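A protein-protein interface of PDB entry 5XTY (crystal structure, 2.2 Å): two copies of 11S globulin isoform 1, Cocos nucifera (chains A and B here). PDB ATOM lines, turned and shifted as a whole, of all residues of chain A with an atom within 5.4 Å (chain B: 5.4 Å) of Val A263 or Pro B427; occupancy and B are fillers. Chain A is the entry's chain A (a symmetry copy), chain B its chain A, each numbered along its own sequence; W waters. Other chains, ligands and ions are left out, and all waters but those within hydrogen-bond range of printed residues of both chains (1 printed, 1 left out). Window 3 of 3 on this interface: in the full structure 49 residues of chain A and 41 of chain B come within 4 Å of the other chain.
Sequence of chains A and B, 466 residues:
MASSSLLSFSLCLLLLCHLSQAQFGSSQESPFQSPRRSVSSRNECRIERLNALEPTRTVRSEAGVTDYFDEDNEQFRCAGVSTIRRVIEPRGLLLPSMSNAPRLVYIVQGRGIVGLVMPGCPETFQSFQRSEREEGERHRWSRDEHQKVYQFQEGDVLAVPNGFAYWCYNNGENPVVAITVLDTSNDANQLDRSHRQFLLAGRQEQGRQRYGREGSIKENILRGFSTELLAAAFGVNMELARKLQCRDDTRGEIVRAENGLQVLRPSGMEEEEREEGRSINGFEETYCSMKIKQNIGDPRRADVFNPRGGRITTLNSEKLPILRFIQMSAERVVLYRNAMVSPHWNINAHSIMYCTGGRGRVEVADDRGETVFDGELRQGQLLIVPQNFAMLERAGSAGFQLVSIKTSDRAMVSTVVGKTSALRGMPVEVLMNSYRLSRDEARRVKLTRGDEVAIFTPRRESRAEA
Water W1 bridges the side-chain carboxylate of Glu B429 (2.4 Å) and the backbone NH of Gln A262 (3.2 Å).
Of the printed residues of chain B, Glu A145 touches Met B426.
Of the printed residues of chain B, His A146 touches Gly B425, Met B426 and Pro B427.
Printed residues of chain B within 4 Å of Leu A261: Glu B429.
Of the printed residues of chain A, Pro B427 touches His A146, Trp A167 and Val A263.
Val B428 touches none of the printed residues of chain A.
Leu B431 touches none of the printed residues of chain A.
The nearest residue of chain A that does not touch Pro B427 is Val A149 (4.1 Å).
The nearest printed residue of chain B that does not touch His A146 is Val B428 (4.9 Å).
Among the printed residues, pairs that only touch across the chains: Glu A145 with Met B426 (3.8 Å), His A146 with Gly B425 (3.1 Å), His A146 with Met B426 (3.2 Å), His A146 with Pro B427 (3.2 Å), Trp A167 with Met B426 (3.8 Å), Trp A167 with Pro B427 (3.4 Å), Leu A261 with Glu B429 (3.5 Å) and Val A263 with Pro B427 (3.5 Å).
Among the printed residues, 10 pairs touch across the chains.
Among the printed residues, no Asp or Glu carboxylate lies within 4 Å of a Lys or Arg side-chain nitrogen of the other chain.
No position is printed for both chains.
Of the 10 pairs that touch across the chains among the printed residues, none has its exchanged pair printed and touching as well.
The backbone NH (N) of Gln A262 sits close to the side-chain carboxylate (OE2) of Glu B429, at 3.1 Å.
The backbone carbonyl oxygen (O) of Gly B425 lies within hydrogen-bond range of the backbone NH (N) of Gln A147 (2.7 Å).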
ATOM      1  N   ILE A 113       6.832  -4.843  24.549  1.00  0.00           N
ATOM      2  CA  ILE A 113       6.455  -5.659  25.689  1.00  0.00           C
ATOM      3  C   ILE A 113       7.382  -5.314  26.833  1.00  0.00           C
ATOM      4  O   ILE A 113       8.535  -4.931  26.625  1.00  0.00           O
ATOM      5  CB  ILE A 113       6.565  -7.157  25.380  1.00  0.00           C
ATOM      6  CG1 ILE A 113       5.881  -7.475  24.062  1.00  0.00           C
ATOM      7  CG2 ILE A 113       5.978  -7.973  26.493  1.00  0.00           C
ATOM      8  CD1 ILE A 113       6.579  -8.555  23.284  1.00  0.00           C
ATOM      9  N   GLU A 145       5.324 -21.589  28.278  1.00  0.00           N
ATOM     10  CA  GLU A 145       4.514 -20.901  29.266  1.00  0.00           C
ATOM     11  C   GLU A 145       5.431 -20.115  30.177  1.00  0.00           C
ATOM     12  O   GLU A 145       6.634 -20.377  30.270  1.00  0.00           O
ATOM     13  CB  GLU A 145       3.659 -21.863  30.082  1.00  0.00           C
ATOM     14  CG  GLU A 145       4.447 -23.004  30.685  1.00  0.00           C
ATOM     15  CD  GLU A 145       3.782 -23.588  31.910  1.00  0.00           C
ATOM     16  OE1 GLU A 145       4.205 -23.257  33.036  1.00  0.00           O
ATOM     17  OE2 GLU A 145       2.836 -24.380  31.741  1.00  0.00           O
ATOM     18  N   HIS A 146       4.822 -19.171  30.882  1.00  0.00           N
ATOM     19  CA  HIS A 146       5.549 -18.110  31.550  1.00  0.00           C
ATOM     20  C   HIS A 146       4.556 -17.136  32.141  1.00  0.00           C
ATOM     21  O   HIS A 146       3.351 -17.292  31.949  1.00  0.00           O
ATOM     22  CB  HIS A 146       6.422 -17.373  30.564  1.00  0.00           C
ATOM     23  CG  HIS A 146       5.635 -16.711  29.488  1.00  0.00           C
ATOM     24  ND1 HIS A 146       5.108 -15.447  29.629  1.00  0.00           N
ATOM     25  CD2 HIS A 146       5.244 -17.152  28.271  1.00  0.00           C
ATOM     26  CE1 HIS A 146       4.446 -15.129  28.533  1.00  0.00           C
ATOM     27  NE2 HIS A 146       4.514 -16.146  27.694  1.00  0.00           N
ATOM     28  N   GLN A 147       5.035 -16.106  32.816  1.00  0.00           N
ATOM     29  CA  GLN A 147       4.058 -15.220  33.411  1.00  0.00           C
ATOM     30  C   GLN A 147       3.585 -14.187  32.413  1.00  0.00           C
ATOM     31  O   GLN A 147       4.228 -13.911  31.401  1.00  0.00           O
ATOM     32  CB  GLN A 147       4.611 -14.521  34.639  1.00  0.00           C
ATOM     33  CG  GLN A 147       4.145 -15.160  35.915  1.00  0.00           C
ATOM     34  CD  GLN A 147       4.373 -14.287  37.115  1.00  0.00           C
ATOM     35  OE1 GLN A 147       4.113 -13.083  37.089  1.00  0.00           O
ATOM     36  NE2 GLN A 147       4.880 -14.889  38.182  1.00  0.00           N
ATOM     37  N   VAL A 149       2.771 -10.958  30.396  1.00  0.00           N
ATOM     38  CA  VAL A 149       3.720  -9.958  29.955  1.00  0.00           C
ATOM     39  C   VAL A 149       2.941  -8.694  29.619  1.00  0.00           C
ATOM     40  O   VAL A 149       1.725  -8.722  29.414  1.00  0.00           O
ATOM     41  CB  VAL A 149       4.514 -10.468  28.750  1.00  0.00           C
ATOM     42  CG1 VAL A 149       5.142 -11.788  29.099  1.00  0.00           C
ATOM     43  CG2 VAL A 149       3.595 -10.647  27.566  1.00  0.00           C
ATOM     44  N   TRP A 167      11.980  -7.774  31.826  1.00  0.00           N
ATOM     45  CA  TRP A 167      12.677  -7.774  30.563  1.00  0.00           C
ATOM     46  C   TRP A 167      11.879  -6.925  29.605  1.00  0.00           C
ATOM     47  O   TRP A 167      10.666  -6.787  29.744  1.00  0.00           O
ATOM     48  CB  TRP A 167      12.837  -9.178  30.013  1.00  0.00           C
ATOM     49  CG  TRP A 167      11.643  -9.989  30.216  1.00  0.00           C
ATOM     50  CD1 TRP A 167      11.373 -10.772  31.277  1.00  0.00           C
ATOM     51  CD2 TRP A 167      10.529 -10.104  29.337  1.00  0.00           C
ATOM     52  NE1 TRP A 167      10.158 -11.383  31.121  1.00  0.00           N
ATOM     53  CE2 TRP A 167       9.623 -10.995  29.929  1.00  0.00           C
ATOM     54  CE3 TRP A 167      10.215  -9.551  28.098  1.00  0.00           C
ATOM     55  CZ2 TRP A 167       8.427 -11.340  29.335  1.00  0.00           C
ATOM     56  CZ3 TRP A 167       9.018  -9.896  27.510  1.00  0.00           C
ATOM     57  CH2 TRP A 167       8.139 -10.776  28.132  1.00  0.00           C
ATOM     58  N   LEU A 261      10.974 -11.976  17.991  1.00  0.00           N
ATOM     59  CA  LEU A 261      10.706 -12.758  19.177  1.00  0.00           C
ATOM     60  C   LEU A 261       9.210 -12.967  19.222  1.00  0.00           C
ATOM     61  O   LEU A 261       8.440 -12.024  19.022  1.00  0.00           O
ATOM     62  CB  LEU A 261      11.195 -12.078  20.451  1.00  0.00           C
ATOM     63  CG  LEU A 261      11.436 -13.043  21.610  1.00  0.00           C
ATOM     64  CD1 LEU A 261      12.382 -12.448  22.607  1.00  0.00           C
ATOM     65  CD2 LEU A 261      10.163 -13.400  22.287  1.00  0.00           C
ATOM     66  N   GLN A 262       8.808 -14.199  19.444  1.00  0.00           N
ATOM     67  CA  GLN A 262       7.410 -14.538  19.580  1.00  0.00           C
ATOM     68  C   GLN A 262       7.170 -14.961  21.012  1.00  0.00           C
ATOM     69  O   GLN A 262       8.018 -15.613  21.625  1.00  0.00           O
ATOM     70  CB  GLN A 262       7.014 -15.651  18.611  1.00  0.00           C
ATOM     71  CG  GLN A 262       6.075 -16.695  19.178  1.00  0.00           C
ATOM     72  CD  GLN A 262       4.688 -16.158  19.398  1.00  0.00           C
ATOM     73  OE1 GLN A 262       4.402 -15.005  19.093  1.00  0.00           O
ATOM     74  NE2 GLN A 262       3.817 -16.978  19.963  1.00  0.00           N
ATOM     75  N   VAL A 263       6.036 -14.550  21.552  1.00  0.00           N
ATOM     76  CA  VAL A 263       5.603 -15.023  22.851  1.00  0.00           C
ATOM     77  C   VAL A 263       4.107 -15.238  22.756  1.00  0.00           C
ATOM     78  O   VAL A 263       3.551 -15.318  21.661  1.00  0.00           O
ATOM     79  CB  VAL A 263       5.965 -14.039  23.972  1.00  0.00           C
ATOM     80  CG1 VAL A 263       7.444 -13.950  24.147  1.00  0.00           C
ATOM     81  CG2 VAL A 263       5.423 -12.684  23.661  1.00  0.00           C
ATOM     82  N   LEU A 264       3.433 -15.298  23.897  1.00  0.00           N
ATOM     83  CA  LEU A 264       2.044 -15.743  23.939  1.00  0.00           C
ATOM     84  C   LEU A 264       1.141 -14.518  24.040  1.00  0.00           C
ATOM     85  O   LEU A 264       0.648 -14.151  25.105  1.00  0.00           O
ATOM     86  CB  LEU A 264       1.845 -16.719  25.096  1.00  0.00           C
ATOM     87  CG  LEU A 264       2.370 -18.155  24.917  1.00  0.00           C
ATOM     88  CD1 LEU A 264       3.855 -18.227  24.583  1.00  0.00           C
ATOM     89  CD2 LEU A 264       2.091 -18.970  26.158  1.00  0.00           C
ATOM     90  N   ARG A 265       0.907 -13.894  22.892  1.00  0.00           N
ATOM     91  CA  ARG A 265       0.232 -12.618  22.775  1.00  0.00           C
ATOM     92  C   ARG A 265      -1.117 -12.762  22.079  1.00  0.00           C
ATOM     93  O   ARG A 265      -1.323 -13.698  21.298  1.00  0.00           O
ATOM     94  CB  ARG A 265       1.108 -11.637  21.991  1.00  0.00           C
ATOM     95  CG  ARG A 265       1.810 -12.266  20.798  1.00  0.00           C
ATOM     96  N   GLY B 425       8.897 -18.159  34.642  1.00  0.00           N
ATOM     97  CA  GLY B 425       7.879 -17.225  34.210  1.00  0.00           C
ATOM     98  C   GLY B 425       8.369 -16.374  33.063  1.00  0.00           C
ATOM     99  O   GLY B 425       7.686 -15.458  32.600  1.00  0.00           O
ATOM    100  N   MET B 426       9.565 -16.663  32.616  1.00  0.00           N
ATOM    101  CA  MET B 426       9.864 -15.929  31.412  1.00  0.00           C
ATOM    102  C   MET B 426       9.519 -16.783  30.202  1.00  0.00           C
ATOM    103  O   MET B 426       9.631 -18.015  30.253  1.00  0.00           O
ATOM    104  CB  MET B 426      11.329 -15.543  31.379  1.00  0.00           C
ATOM    105  CG  MET B 426      11.757 -14.829  32.631  1.00  0.00           C
ATOM    106  SD  MET B 426      13.281 -13.882  32.494  1.00  0.00           S
ATOM    107  CE  MET B 426      14.509 -15.168  32.359  1.00  0.00           C
ATOM    108  N   PRO B 427       9.044 -16.137  29.144  1.00  0.00           N
ATOM    109  CA  PRO B 427       8.691 -16.864  27.925  1.00  0.00           C
ATOM    110  C   PRO B 427       9.887 -17.602  27.356  1.00  0.00           C
ATOM    111  O   PRO B 427      11.041 -17.240  27.583  1.00  0.00           O
ATOM    112  CB  PRO B 427       8.219 -15.759  26.981  1.00  0.00           C
ATOM    113  CG  PRO B 427       7.844 -14.619  27.880  1.00  0.00           C
ATOM    114  CD  PRO B 427       8.733 -14.702  29.059  1.00  0.00           C
ATOM    115  N   VAL B 428       9.594 -18.658  26.599  1.00  0.00           N
ATOM    116  CA  VAL B 428      10.651 -19.575  26.188  1.00  0.00           C
ATOM    117  C   VAL B 428      11.677 -18.862  25.327  1.00  0.00           C
ATOM    118  O   VAL B 428      12.885 -19.000  25.533  1.00  0.00           O
ATOM    119  CB  VAL B 428      10.060 -20.800  25.475  1.00  0.00           C
ATOM    120  CG1 VAL B 428       9.319 -20.419  24.234  1.00  0.00           C
ATOM    121  CG2 VAL B 428      11.141 -21.793  25.161  1.00  0.00           C
ATOM    122  N   GLU B 429      11.222 -18.070  24.365  1.00  0.00           N
ATOM    123  CA  GLU B 429      12.195 -17.354  23.556  1.00  0.00           C
ATOM    124  C   GLU B 429      12.985 -16.382  24.409  1.00  0.00           C
ATOM    125  O   GLU B 429      14.175 -16.157  24.158  1.00  0.00           O
ATOM    126  CB  GLU B 429      11.516 -16.640  22.397  1.00  0.00           C
ATOM    127  CG  GLU B 429      10.935 -17.609  21.375  1.00  0.00           C
ATOM    128  CD  GLU B 429      10.496 -16.962  20.096  1.00  0.00           C
ATOM    129  OE1 GLU B 429      11.279 -16.175  19.538  1.00  0.00           O
ATOM    130  OE2 GLU B 429       9.394 -17.277  19.615  1.00  0.00           O
ATOM    131  N   VAL B 430      12.356 -15.843  25.455  1.00  0.00           N
ATOM    132  CA  VAL B 430      13.061 -14.981  26.387  1.00  0.00           C
ATOM    133  C   VAL B 430      14.169 -15.735  27.084  1.00  0.00           C
ATOM    134  O   VAL B 430      15.171 -15.144  27.483  1.00  0.00           O
ATOM    135  CB  VAL B 430      12.066 -14.385  27.391  1.00  0.00           C
ATOM    136  CG1 VAL B 430      12.784 -13.508  28.390  1.00  0.00           C
ATOM    137  CG2 VAL B 430      11.012 -13.587  26.651  1.00  0.00           C
ATOM    138  N   LEU B 431      14.034 -17.042  27.215  1.00  0.00           N
ATOM    139  CA  LEU B 431      15.148 -17.803  27.745  1.00  0.00           C
ATOM    140  C   LEU B 431      16.206 -18.055  26.677  1.00  0.00           C
ATOM    141  O   LEU B 431      17.400 -18.086  26.984  1.00  0.00           O
ATOM    142  CB  LEU B 431      14.619 -19.105  28.349  1.00  0.00           C
ATOM    143  CG  LEU B 431      13.515 -18.907  29.405  1.00  0.00           C
ATOM    144  CD1 LEU B 431      12.773 -20.193  29.755  1.00  0.00           C
ATOM    145  CD2 LEU B 431      14.092 -18.285  30.650  1.00  0.00           C
ATOM    146  N   MET B 432      15.803 -18.179  25.416  1.00  0.00           N
ATOM    147  CA  MET B 432      16.766 -18.516  24.375  1.00  0.00           C
ATOM    148  C   MET B 432      17.600 -17.335  23.927  1.00  0.00           C
ATOM    149  O   MET B 432      18.762 -17.507  23.554  1.00  0.00           O
ATOM    150  CB  MET B 432      16.054 -19.073  23.159  1.00  0.00           C
ATOM    151  CG  MET B 432      14.977 -20.034  23.478  1.00  0.00           C
ATOM    152  SD  MET B 432      14.334 -20.584  21.928  1.00  0.00           S
ATOM    153  CE  MET B 432      12.607 -20.643  22.292  1.00  0.00           C
HETATM  154  O   HOH W   1       9.777 -16.507  17.374  1.00  0.00           O
